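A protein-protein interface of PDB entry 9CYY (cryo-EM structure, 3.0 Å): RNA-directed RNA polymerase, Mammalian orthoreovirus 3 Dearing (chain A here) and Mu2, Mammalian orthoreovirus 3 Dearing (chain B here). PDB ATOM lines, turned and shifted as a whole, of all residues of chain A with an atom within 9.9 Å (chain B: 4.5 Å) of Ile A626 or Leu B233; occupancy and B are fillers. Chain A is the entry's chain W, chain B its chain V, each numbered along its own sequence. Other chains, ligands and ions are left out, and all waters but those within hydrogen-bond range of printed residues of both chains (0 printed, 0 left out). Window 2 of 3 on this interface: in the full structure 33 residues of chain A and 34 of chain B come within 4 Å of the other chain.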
ATOM      1  N   ILE A 408      25.031  -3.169 -26.581  1.00  0.00           N
ATOM      2  CA  ILE A 408      25.619  -2.114 -25.762  1.00  0.00           C
ATOM      3  C   ILE A 408      24.464  -1.475 -25.006  1.00  0.00           C
ATOM      4  O   ILE A 408      23.469  -1.059 -25.614  1.00  0.00           O
ATOM      5  CB  ILE A 408      26.400  -1.085 -26.593  1.00  0.00           C
ATOM      6  CG1 ILE A 408      25.493  -0.366 -27.593  1.00  0.00           C
ATOM      7  CG2 ILE A 408      27.547  -1.739 -27.316  1.00  0.00           C
ATOM      8  CD1 ILE A 408      26.142   0.798 -28.265  1.00  0.00           C
ATOM      9  N   GLY A 409      24.570  -1.423 -23.688  1.00  0.00           N
ATOM     10  CA  GLY A 409      23.365  -1.155 -22.929  1.00  0.00           C
ATOM     11  C   GLY A 409      22.396  -2.278 -23.233  1.00  0.00           C
ATOM     12  O   GLY A 409      22.544  -3.408 -22.750  1.00  0.00           O
ATOM     13  N   PHE A 502      15.577  11.199 -10.334  1.00  0.00           N
ATOM     14  CA  PHE A 502      15.381  10.496 -11.597  1.00  0.00           C
ATOM     15  C   PHE A 502      15.374   8.989 -11.387  1.00  0.00           C
ATOM     16  O   PHE A 502      14.670   8.262 -12.094  1.00  0.00           O
ATOM     17  CB  PHE A 502      16.461  10.893 -12.601  1.00  0.00           C
ATOM     18  CG  PHE A 502      16.437  10.080 -13.861  1.00  0.00           C
ATOM     19  CD1 PHE A 502      15.439  10.271 -14.802  1.00  0.00           C
ATOM     20  CD2 PHE A 502      17.406   9.122 -14.103  1.00  0.00           C
ATOM     21  CE1 PHE A 502      15.412   9.525 -15.963  1.00  0.00           C
ATOM     22  CE2 PHE A 502      17.383   8.373 -15.262  1.00  0.00           C
ATOM     23  CZ  PHE A 502      16.384   8.576 -16.193  1.00  0.00           C
ATOM     24  N   HIS A 607      22.452   7.086 -30.421  1.00  0.00           N
ATOM     25  CA  HIS A 607      23.169   6.772 -29.190  1.00  0.00           C
ATOM     26  C   HIS A 607      24.676   6.811 -29.409  1.00  0.00           C
ATOM     27  O   HIS A 607      25.430   7.238 -28.526  1.00  0.00           O
ATOM     28  CB  HIS A 607      22.729   5.409 -28.658  1.00  0.00           C
ATOM     29  CG  HIS A 607      23.266   5.091 -27.297  1.00  0.00           C
ATOM     30  ND1 HIS A 607      22.635   5.491 -26.137  1.00  0.00           N
ATOM     31  CD2 HIS A 607      24.370   4.411 -26.909  1.00  0.00           C
ATOM     32  CE1 HIS A 607      23.330   5.072 -25.095  1.00  0.00           C
ATOM     33  NE2 HIS A 607      24.387   4.415 -25.535  1.00  0.00           N
ATOM     34  N   ILE A 615      30.369  13.797 -22.892  1.00  0.00           N
ATOM     35  CA  ILE A 615      30.872  12.765 -21.995  1.00  0.00           C
ATOM     36  C   ILE A 615      30.728  13.185 -20.539  1.00  0.00           C
ATOM     37  O   ILE A 615      31.196  14.250 -20.126  1.00  0.00           O
ATOM     38  CB  ILE A 615      32.336  12.437 -22.330  1.00  0.00           C
ATOM     39  CG1 ILE A 615      32.450  11.948 -23.771  1.00  0.00           C
ATOM     40  CG2 ILE A 615      32.878  11.387 -21.377  1.00  0.00           C
ATOM     41  CD1 ILE A 615      31.660  10.692 -24.050  1.00  0.00           C
ATOM     42  N   GLY A 616      30.069  12.328 -19.758  1.00  0.00           N
ATOM     43  CA  GLY A 616      30.002  12.478 -18.318  1.00  0.00           C
ATOM     44  C   GLY A 616      29.369  13.765 -17.829  1.00  0.00           C
ATOM     45  O   GLY A 616      29.928  14.435 -16.954  1.00  0.00           O
ATOM     46  N   PRO A 623      20.683  12.590 -14.973  1.00  0.00           N
ATOM     47  CA  PRO A 623      22.122  12.470 -14.739  1.00  0.00           C
ATOM     48  C   PRO A 623      22.767  11.452 -15.674  1.00  0.00           C
ATOM     49  O   PRO A 623      22.099  10.641 -16.317  1.00  0.00           O
ATOM     50  CB  PRO A 623      22.191  11.991 -13.283  1.00  0.00           C
ATOM     51  CG  PRO A 623      20.949  11.197 -13.110  1.00  0.00           C
ATOM     52  CD  PRO A 623      19.896  11.886 -13.944  1.00  0.00           C
ATOM     53  N   ALA A 624      24.094  11.520 -15.737  1.00  0.00           N
ATOM     54  CA  ALA A 624      24.878  10.526 -16.447  1.00  0.00           C
ATOM     55  C   ALA A 624      24.907   9.238 -15.631  1.00  0.00           C
ATOM     56  O   ALA A 624      24.509   9.205 -14.464  1.00  0.00           O
ATOM     57  CB  ALA A 624      26.288  11.049 -16.715  1.00  0.00           C
ATOM     58  N   SER A 625      25.383   8.162 -16.238  1.00  0.00           N
ATOM     59  CA  SER A 625      25.366   6.864 -15.573  1.00  0.00           C
ATOM     60  C   SER A 625      26.436   5.977 -16.200  1.00  0.00           C
ATOM     61  O   SER A 625      27.307   6.446 -16.944  1.00  0.00           O
ATOM     62  CB  SER A 625      23.977   6.226 -15.642  1.00  0.00           C
ATOM     63  OG  SER A 625      23.765   5.595 -16.892  1.00  0.00           O
ATOM     64  N   ILE A 626      26.362   4.688 -15.887  1.00  0.00           N
ATOM     65  CA  ILE A 626      27.361   3.688 -16.239  1.00  0.00           C
ATOM     66  C   ILE A 626      26.660   2.362 -16.511  1.00  0.00           C
ATOM     67  O   ILE A 626      25.879   1.882 -15.683  1.00  0.00           O
ATOM     68  CB  ILE A 626      28.427   3.572 -15.124  1.00  0.00           C
ATOM     69  CG1 ILE A 626      29.568   2.624 -15.516  1.00  0.00           C
ATOM     70  CG2 ILE A 626      27.796   3.315 -13.754  1.00  0.00           C
ATOM     71  CD1 ILE A 626      30.404   3.086 -16.645  1.00  0.00           C
ATOM     72  N   VAL A 627      26.920   1.782 -17.685  1.00  0.00           N
ATOM     73  CA  VAL A 627      26.237   0.580 -18.146  1.00  0.00           C
ATOM     74  C   VAL A 627      27.259  -0.388 -18.739  1.00  0.00           C
ATOM     75  O   VAL A 627      28.457  -0.116 -18.780  1.00  0.00           O
ATOM     76  CB  VAL A 627      25.126   0.889 -19.171  1.00  0.00           C
ATOM     77  CG1 VAL A 627      24.032   1.740 -18.542  1.00  0.00           C
ATOM     78  CG2 VAL A 627      25.711   1.568 -20.397  1.00  0.00           C
ATOM     79  N   ASN A 628      26.756  -1.524 -19.219  1.00  0.00           N
ATOM     80  CA  ASN A 628      27.572  -2.641 -19.672  1.00  0.00           C
ATOM     81  C   ASN A 628      27.738  -2.618 -21.188  1.00  0.00           C
ATOM     82  O   ASN A 628      26.864  -2.158 -21.924  1.00  0.00           O
ATOM     83  CB  ASN A 628      26.943  -3.969 -19.238  1.00  0.00           C
ATOM     84  CG  ASN A 628      27.846  -5.164 -19.497  1.00  0.00           C
ATOM     85  OD1 ASN A 628      28.947  -5.029 -20.029  1.00  0.00           O
ATOM     86  ND2 ASN A 628      27.376  -6.346 -19.119  1.00  0.00           N
ATOM     87  N   ASP A 629      28.882  -3.126 -21.643  1.00  0.00           N
ATOM     88  CA  ASP A 629      29.225  -3.205 -23.056  1.00  0.00           C
ATOM     89  C   ASP A 629      29.736  -4.599 -23.382  1.00  0.00           C
ATOM     90  O   ASP A 629      30.655  -5.093 -22.728  1.00  0.00           O
ATOM     91  CB  ASP A 629      30.290  -2.161 -23.413  1.00  0.00           C
ATOM     92  CG  ASP A 629      30.542  -2.058 -24.905  1.00  0.00           C
ATOM     93  OD1 ASP A 629      29.922  -2.816 -25.678  1.00  0.00           O
ATOM     94  OD2 ASP A 629      31.371  -1.215 -25.307  1.00  0.00           O
ATOM     95  N   ARG A 636      33.647  -8.141 -22.155  1.00  0.00           N
ATOM     96  CA  ARG A 636      32.438  -7.360 -21.906  1.00  0.00           C
ATOM     97  C   ARG A 636      32.604  -6.529 -20.630  1.00  0.00           C
ATOM     98  O   ARG A 636      32.476  -7.008 -19.505  1.00  0.00           O
ATOM     99  CB  ARG A 636      31.178  -8.284 -21.928  1.00  0.00           C
ATOM    100  CG  ARG A 636      31.038  -9.462 -20.965  1.00  0.00           C
ATOM    101  CD  ARG A 636      30.380  -9.118 -19.638  1.00  0.00           C
ATOM    102  NE  ARG A 636      30.147 -10.330 -18.862  1.00  0.00           N
ATOM    103  CZ  ARG A 636      29.702 -10.343 -17.616  1.00  0.00           C
ATOM    104  NH1 ARG A 636      29.461  -9.224 -16.956  1.00  0.00           N
ATOM    105  NH2 ARG A 636      29.499 -11.509 -17.009  1.00  0.00           N
ATOM    106  N   ALA A 637      32.921  -5.249 -20.837  1.00  0.00           N
ATOM    107  CA  ALA A 637      33.246  -4.301 -19.783  1.00  0.00           C
ATOM    108  C   ALA A 637      32.169  -3.219 -19.653  1.00  0.00           C
ATOM    109  O   ALA A 637      31.085  -3.303 -20.233  1.00  0.00           O
ATOM    110  CB  ALA A 637      34.603  -3.664 -20.064  1.00  0.00           C
ATOM    111  N   ALA A 638      32.488  -2.188 -18.876  1.00  0.00           N
ATOM    112  CA  ALA A 638      31.545  -1.136 -18.521  1.00  0.00           C
ATOM    113  C   ALA A 638      31.913   0.174 -19.212  1.00  0.00           C
ATOM    114  O   ALA A 638      33.054   0.634 -19.109  1.00  0.00           O
ATOM    115  CB  ALA A 638      31.526  -0.939 -17.005  1.00  0.00           C
ATOM    116  N   ARG A 639      30.931   0.788 -19.902  1.00  0.00           N
ATOM    117  CA  ARG A 639      31.116   2.067 -20.578  1.00  0.00           C
ATOM    118  C   ARG A 639      30.265   3.158 -19.939  1.00  0.00           C
ATOM    119  O   ARG A 639      29.083   2.935 -19.654  1.00  0.00           O
ATOM    120  CB  ARG A 639      30.761   1.976 -22.068  1.00  0.00           C
ATOM    121  CG  ARG A 639      31.614   1.028 -22.898  1.00  0.00           C
ATOM    122  CD  ARG A 639      33.001   1.587 -23.198  1.00  0.00           C
ATOM    123  NE  ARG A 639      33.894   1.551 -22.047  1.00  0.00           N
ATOM    124  CZ  ARG A 639      34.516   0.464 -21.615  1.00  0.00           C
ATOM    125  NH1 ARG A 639      34.361  -0.705 -22.213  1.00  0.00           N
ATOM    126  NH2 ARG A 639      35.303   0.549 -20.546  1.00  0.00           N
ATOM    127  N   PRO A 640      30.835   4.344 -19.693  1.00  0.00           N
ATOM    128  CA  PRO A 640      30.040   5.441 -19.126  1.00  0.00           C
ATOM    129  C   PRO A 640      29.235   6.183 -20.179  1.00  0.00           C
ATOM    130  O   PRO A 640      29.736   6.473 -21.269  1.00  0.00           O
ATOM    131  CB  PRO A 640      31.101   6.344 -18.485  1.00  0.00           C
ATOM    132  CG  PRO A 640      32.328   6.109 -19.297  1.00  0.00           C
ATOM    133  CD  PRO A 640      32.255   4.704 -19.847  1.00  0.00           C
ATOM    134  N   ILE A 641      27.984   6.499 -19.857  1.00  0.00           N
ATOM    135  CA  ILE A 641      27.093   7.153 -20.806  1.00  0.00           C
ATOM    136  C   ILE A 641      26.672   8.517 -20.274  1.00  0.00           C
ATOM    137  O   ILE A 641      26.720   8.767 -19.065  1.00  0.00           O
ATOM    138  CB  ILE A 641      25.873   6.266 -21.112  1.00  0.00           C
ATOM    139  CG1 ILE A 641      24.990   6.107 -19.875  1.00  0.00           C
ATOM    140  CG2 ILE A 641      26.321   4.915 -21.645  1.00  0.00           C
ATOM    141  CD1 ILE A 641      23.866   5.118 -20.065  1.00  0.00           C
ATOM    142  N   SER A 642      26.263   9.403 -21.174  1.00  0.00           N
ATOM    143  CA  SER A 642      25.923  10.778 -20.843  1.00  0.00           C
ATOM    144  C   SER A 642      24.444  10.899 -20.495  1.00  0.00           C
ATOM    145  O   SER A 642      23.733   9.908 -20.327  1.00  0.00           O
ATOM    146  CB  SER A 642      26.265  11.704 -22.010  1.00  0.00           C
ATOM    147  OG  SER A 642      25.646  11.267 -23.207  1.00  0.00           O
ATOM    148  N   GLY A 643      23.985  12.148 -20.389  1.00  0.00           N
ATOM    149  CA  GLY A 643      22.571  12.381 -20.144  1.00  0.00           C
ATOM    150  C   GLY A 643      21.700  11.898 -21.287  1.00  0.00           C
ATOM    151  O   GLY A 643      20.750  11.134 -21.084  1.00  0.00           O
ATOM    152  N   GLN A 645      22.624   9.832 -23.599  1.00  0.00           N
ATOM    153  CA  GLN A 645      22.844   8.401 -23.767  1.00  0.00           C
ATOM    154  C   GLN A 645      22.002   7.587 -22.794  1.00  0.00           C
ATOM    155  O   GLN A 645      21.386   6.594 -23.191  1.00  0.00           O
ATOM    156  CB  GLN A 645      24.328   8.087 -23.601  1.00  0.00           C
ATOM    157  CG  GLN A 645      25.100   8.051 -24.903  1.00  0.00           C
ATOM    158  CD  GLN A 645      26.558   7.700 -24.704  1.00  0.00           C
ATOM    159  OE1 GLN A 645      27.234   8.270 -23.849  1.00  0.00           O
ATOM    160  NE2 GLN A 645      27.053   6.757 -25.495  1.00  0.00           N
ATOM    161  N   ASN A 646      21.940   8.004 -21.528  1.00  0.00           N
ATOM    162  CA  ASN A 646      21.076   7.334 -20.559  1.00  0.00           C
ATOM    163  C   ASN A 646      19.611   7.462 -20.957  1.00  0.00           C
ATOM    164  O   ASN A 646      18.833   6.504 -20.844  1.00  0.00           O
ATOM    165  CB  ASN A 646      21.309   7.926 -19.168  1.00  0.00           C
ATOM    166  CG  ASN A 646      20.751   7.057 -18.062  1.00  0.00           C
ATOM    167  OD1 ASN A 646      20.182   5.998 -18.315  1.00  0.00           O
ATOM    168  ND2 ASN A 646      20.900   7.512 -16.824  1.00  0.00           N
ATOM    169  N   MET A 647      19.216   8.648 -21.420  1.00  0.00           N
ATOM    170  CA  MET A 647      17.830   8.874 -21.808  1.00  0.00           C
ATOM    171  C   MET A 647      17.434   7.989 -22.987  1.00  0.00           C
ATOM    172  O   MET A 647      16.354   7.386 -22.992  1.00  0.00           O
ATOM    173  CB  MET A 647      17.644  10.356 -22.124  1.00  0.00           C
ATOM    174  CG  MET A 647      16.242  10.771 -22.419  1.00  0.00           C
ATOM    175  SD  MET A 647      16.112  12.534 -22.764  1.00  0.00           S
ATOM    176  CE  MET A 647      16.375  13.224 -21.136  1.00  0.00           C
ATOM    177  N   GLN A 649      18.950   5.189 -23.716  1.00  0.00           N
ATOM    178  CA  GLN A 649      18.982   3.826 -23.205  1.00  0.00           C
ATOM    179  C   GLN A 649      17.656   3.450 -22.565  1.00  0.00           C
ATOM    180  O   GLN A 649      17.174   2.325 -22.738  1.00  0.00           O
ATOM    181  CB  GLN A 649      20.122   3.681 -22.195  1.00  0.00           C
ATOM    182  CG  GLN A 649      20.533   2.253 -21.917  1.00  0.00           C
ATOM    183  CD  GLN A 649      21.147   1.589 -23.130  1.00  0.00           C
ATOM    184  OE1 GLN A 649      20.537   0.724 -23.753  1.00  0.00           O
ATOM    185  NE2 GLN A 649      22.359   2.002 -23.480  1.00  0.00           N
ATOM    186  N   HIS A 650      17.053   4.378 -21.824  1.00  0.00           N
ATOM    187  CA  HIS A 650      15.763   4.108 -21.198  1.00  0.00           C
ATOM    188  C   HIS A 650      14.628   4.111 -22.220  1.00  0.00           C
ATOM    189  O   HIS A 650      13.659   3.355 -22.092  1.00  0.00           O
ATOM    190  CB  HIS A 650      15.499   5.121 -20.084  1.00  0.00           C
ATOM    191  CG  HIS A 650      16.386   4.947 -18.890  1.00  0.00           C
ATOM    192  ND1 HIS A 650      16.431   5.858 -17.858  1.00  0.00           N
ATOM    193  CD2 HIS A 650      17.260   3.966 -18.563  1.00  0.00           C
ATOM    194  CE1 HIS A 650      17.294   5.447 -16.946  1.00  0.00           C
ATOM    195  NE2 HIS A 650      17.812   4.301 -17.350  1.00  0.00           N
ATOM    196  N   ALA B  56      33.821  10.047 -14.672  1.00  0.00           N
ATOM    197  CA  ALA B  56      34.032   8.846 -13.868  1.00  0.00           C
ATOM    198  C   ALA B  56      35.504   8.641 -13.532  1.00  0.00           C
ATOM    199  O   ALA B  56      35.841   8.261 -12.402  1.00  0.00           O
ATOM    200  CB  ALA B  56      33.478   7.623 -14.599  1.00  0.00           C
ATOM    201  N   ILE B  60      37.135   8.204  -9.758  1.00  0.00           N
ATOM    202  CA  ILE B  60      37.620   6.885  -9.363  1.00  0.00           C
ATOM    203  C   ILE B  60      39.082   6.958  -8.940  1.00  0.00           C
ATOM    204  O   ILE B  60      39.475   6.397  -7.908  1.00  0.00           O
ATOM    205  CB  ILE B  60      37.411   5.873 -10.504  1.00  0.00           C
ATOM    206  CG1 ILE B  60      35.924   5.555 -10.668  1.00  0.00           C
ATOM    207  CG2 ILE B  60      38.206   4.604 -10.244  1.00  0.00           C
ATOM    208  CD1 ILE B  60      35.647   4.385 -11.583  1.00  0.00           C
ATOM    209  N   GLU B 229      27.141  -2.955 -11.256  1.00  0.00           N
ATOM    210  CA  GLU B 229      27.759  -2.312 -12.407  1.00  0.00           C
ATOM    211  C   GLU B 229      28.733  -1.213 -11.983  1.00  0.00           C
ATOM    212  O   GLU B 229      29.799  -1.052 -12.592  1.00  0.00           O
ATOM    213  CB  GLU B 229      26.659  -1.770 -13.318  1.00  0.00           C
ATOM    214  CG  GLU B 229      27.027  -1.735 -14.777  1.00  0.00           C
ATOM    215  CD  GLU B 229      27.905  -0.567 -15.090  1.00  0.00           C
ATOM    216  OE1 GLU B 229      27.861   0.399 -14.312  1.00  0.00           O
ATOM    217  OE2 GLU B 229      28.633  -0.608 -16.097  1.00  0.00           O
ATOM    218  N   PHE B 230      28.387  -0.443 -10.947  1.00  0.00           N
ATOM    219  CA  PHE B 230      29.300   0.589 -10.459  1.00  0.00           C
ATOM    220  C   PHE B 230      30.581  -0.029  -9.913  1.00  0.00           C
ATOM    221  O   PHE B 230      31.687   0.473 -10.160  1.00  0.00           O
ATOM    222  CB  PHE B 230      28.616   1.440  -9.388  1.00  0.00           C
ATOM    223  CG  PHE B 230      27.675   2.473  -9.939  1.00  0.00           C
ATOM    224  CD1 PHE B 230      26.445   2.106 -10.457  1.00  0.00           C
ATOM    225  CD2 PHE B 230      28.023   3.814  -9.945  1.00  0.00           C
ATOM    226  CE1 PHE B 230      25.577   3.057 -10.962  1.00  0.00           C
ATOM    227  CE2 PHE B 230      27.162   4.768 -10.451  1.00  0.00           C
ATOM    228  CZ  PHE B 230      25.937   4.389 -10.959  1.00  0.00           C
ATOM    229  N   ILE B 231      30.450  -1.121  -9.161  1.00  0.00           N
ATOM    230  CA  ILE B 231      31.627  -1.827  -8.667  1.00  0.00           C
ATOM    231  C   ILE B 231      32.425  -2.404  -9.826  1.00  0.00           C
ATOM    232  O   ILE B 231      33.662  -2.436  -9.793  1.00  0.00           O
ATOM    233  CB  ILE B 231      31.216  -2.914  -7.659  1.00  0.00           C
ATOM    234  CG1 ILE B 231      30.496  -2.276  -6.471  1.00  0.00           C
ATOM    235  CG2 ILE B 231      32.427  -3.708  -7.202  1.00  0.00           C
ATOM    236  CD1 ILE B 231      29.794  -3.267  -5.584  1.00  0.00           C
ATOM    237  N   LYS B 232      31.733  -2.870 -10.869  1.00  0.00           N
ATOM    238  CA  LYS B 232      32.429  -3.347 -12.061  1.00  0.00           C
ATOM    239  C   LYS B 232      33.292  -2.246 -12.661  1.00  0.00           C
ATOM    240  O   LYS B 232      34.464  -2.466 -12.985  1.00  0.00           O
ATOM    241  CB  LYS B 232      31.417  -3.850 -13.091  1.00  0.00           C
ATOM    242  CG  LYS B 232      32.037  -4.381 -14.374  1.00  0.00           C
ATOM    243  CD  LYS B 232      30.961  -4.701 -15.396  1.00  0.00           C
ATOM    244  CE  LYS B 232      30.286  -6.016 -15.084  1.00  0.00           C
ATOM    245  NZ  LYS B 232      29.320  -6.396 -16.147  1.00  0.00           N
ATOM    246  N   LEU B 233      32.723  -1.046 -12.807  1.00  0.00           N
ATOM    247  CA  LEU B 233      33.489   0.080 -13.337  1.00  0.00           C
ATOM    248  C   LEU B 233      34.683   0.413 -12.456  1.00  0.00           C
ATOM    249  O   LEU B 233      35.794   0.639 -12.956  1.00  0.00           O
ATOM    250  CB  LEU B 233      32.605   1.316 -13.473  1.00  0.00           C
ATOM    251  CG  LEU B 233      33.383   2.487 -14.082  1.00  0.00           C
ATOM    252  CD1 LEU B 233      33.856   2.176 -15.498  1.00  0.00           C
ATOM    253  CD2 LEU B 233      32.615   3.798 -14.012  1.00  0.00           C
ATOM    254  N   PHE B 234      34.466   0.480 -11.142  1.00  0.00           N
ATOM    255  CA  PHE B 234      35.549   0.840 -10.234  1.00  0.00           C
ATOM    256  C   PHE B 234      36.690  -0.165 -10.325  1.00  0.00           C
ATOM    257  O   PHE B 234      37.863   0.213 -10.449  1.00  0.00           O
ATOM    258  CB  PHE B 234      35.017   0.939  -8.805  1.00  0.00           C
ATOM    259  CG  PHE B 234      35.961   1.607  -7.851  1.00  0.00           C
ATOM    260  CD1 PHE B 234      36.985   0.896  -7.253  1.00  0.00           C
ATOM    261  CD2 PHE B 234      35.826   2.951  -7.557  1.00  0.00           C
ATOM    262  CE1 PHE B 234      37.851   1.512  -6.377  1.00  0.00           C
ATOM    263  CE2 PHE B 234      36.691   3.571  -6.684  1.00  0.00           C
ATOM    264  CZ  PHE B 234      37.704   2.852  -6.093  1.00  0.00           C
ATOM    265  N   TYR B 235      36.357  -1.457 -10.279  1.00  0.00           N
ATOM    266  CA  TYR B 235      37.384  -2.488 -10.362  1.00  0.00           C
ATOM    267  C   TYR B 235      38.090  -2.461 -11.709  1.00  0.00           C
ATOM    268  O   TYR B 235      39.313  -2.629 -11.775  1.00  0.00           O
ATOM    269  CB  TYR B 235      36.772  -3.860 -10.095  1.00  0.00           C
ATOM    270  CG  TYR B 235      36.780  -4.235  -8.635  1.00  0.00           C
ATOM    271  CD1 TYR B 235      36.058  -3.502  -7.703  1.00  0.00           C
ATOM    272  CD2 TYR B 235      37.528  -5.311  -8.184  1.00  0.00           C
ATOM    273  CE1 TYR B 235      36.072  -3.842  -6.367  1.00  0.00           C
ATOM    274  CE2 TYR B 235      37.548  -5.656  -6.851  1.00  0.00           C
ATOM    275  CZ  TYR B 235      36.820  -4.920  -5.947  1.00  0.00           C
ATOM    276  OH  TYR B 235      36.841  -5.264  -4.618  1.00  0.00           O
ATOM    277  N   GLN B 236      37.344  -2.245 -12.796  1.00  0.00           N
ATOM    278  CA  GLN B 236      37.968  -2.162 -14.111  1.00  0.00           C
ATOM    279  C   GLN B 236      38.987  -1.037 -14.168  1.00  0.00           C
ATOM    280  O   GLN B 236      40.124  -1.237 -14.608  1.00  0.00           O
ATOM    281  CB  GLN B 236      36.912  -1.961 -15.196  1.00  0.00           C
ATOM    282  CG  GLN B 236      37.512  -1.951 -16.589  1.00  0.00           C
ATOM    283  CD  GLN B 236      36.481  -1.807 -17.683  1.00  0.00           C
ATOM    284  OE1 GLN B 236      35.286  -1.677 -17.418  1.00  0.00           O
ATOM    285  NE2 GLN B 236      36.944  -1.802 -18.927  1.00  0.00           N
ATOM    286  N   ARG B 237      38.595   0.161 -13.729  1.00  0.00           N
ATOM    287  CA  ARG B 237      39.507   1.296 -13.800  1.00  0.00           C
ATOM    288  C   ARG B 237      40.735   1.070 -12.927  1.00  0.00           C
ATOM    289  O   ARG B 237      41.870   1.329 -13.352  1.00  0.00           O
ATOM    290  CB  ARG B 237      38.781   2.577 -13.391  1.00  0.00           C
ATOM    291  CG  ARG B 237      39.599   3.845 -13.557  1.00  0.00           C
ATOM    292  CD  ARG B 237      39.813   4.179 -15.023  1.00  0.00           C
ATOM    293  NE  ARG B 237      40.491   5.458 -15.195  1.00  0.00           N
ATOM    294  CZ  ARG B 237      40.932   5.922 -16.356  1.00  0.00           C
ATOM    295  NH1 ARG B 237      40.789   5.232 -17.476  1.00  0.00           N
ATOM    296  NH2 ARG B 237      41.532   7.108 -16.395  1.00  0.00           N
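The side-chain amide nitrogen (NE2) of Gln B236 lies close to the guanidinium group (NH2) of Arg A639. The guanidinium group (NH1) of Arg A636 lies close to the side-chain amino group (NZ) of Lys B232, at 2.9 Å. O of Ile A626 lies close to OE1 of Glu B229. OE1 of Gln B236 lies within hydrogen-bond range of N of Ala A638 (3.2 Å). OE2 of Glu B229 lies close to N of Val A627.
OD1 of Asn A628 sits close to O of Ala A637 (2.8 Å). The backbone carbonyl oxygen (O) of Val A627 is in hydrogen-bond range of the backbone NH (N) of Arg A639 (2.9 Å). The backbone carbonyl oxygen (O) of Ala A637 sits at hydrogen-bond distance from the backbone NH (N) of Asp A629 (2.6 Å). The backbone NH (N) of Gly A409 is in hydrogen-bond range of the backbone carbonyl oxygen (O) of Asn A628, at 3.0 Å.
CZ of Phe B230 touches CG2 of Ile A626 (3.5 Å). CD1 of Ile A626 touches CD2 of Leu B233 (3.5 Å). Glu B229 touches Asn A628. Asn A628 touches Lys B232. NE2 of Gln B236 touches CB of Ala A637 (3.2 Å). Ala A638 touches Glu B229.
Printed residues of chain B within 4 Å of Ile A626: Glu B229 (2.8 Å), Phe B230 (3.5 Å) and Leu B233 (3.5 Å). Of the printed residues of chain A, Leu B233 touches Ile A626 (3.5 Å). Phe B230 touches one residue of chain A. Of the printed residues of chain A, Glu B229 touches Ile A626 (2.8 Å), Val A627 (2.7 Å), Asn A628 (3.8 Å) and Ala A638 (3.1 Å). Of the printed residues of chain B, Val A627 touches Glu B229. Met A647 touches none of the printed residues of chain B. Ile B60 touches none of the printed residues of chain A. The nearest printed residue of chain B that does not touch Ile A626 is Ala B56 (5.8 Å).
Of the 26 printed residues of chain A, 7 touch a printed residue of chain B. Hydrophobic or aromatic side chains of chain A within 4 Å of the printed part of chain B: Ile A626, Ala A637 and Ala A638. Printed residues of chain B that touch a printed residue of chain A: Glu B229, Phe B230, Lys B232, Leu B233 and Gln B236. Hydrophobic or aromatic side chains of chain B that line the printed part of chain A: Phe B230 and Leu B233. Among the printed residues, 11 pairs touch across the chains. Among the printed residues, no Asp or Glu carboxylate lies within 4 Å of a Lys or Arg side-chain nitrogen of the other chain.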
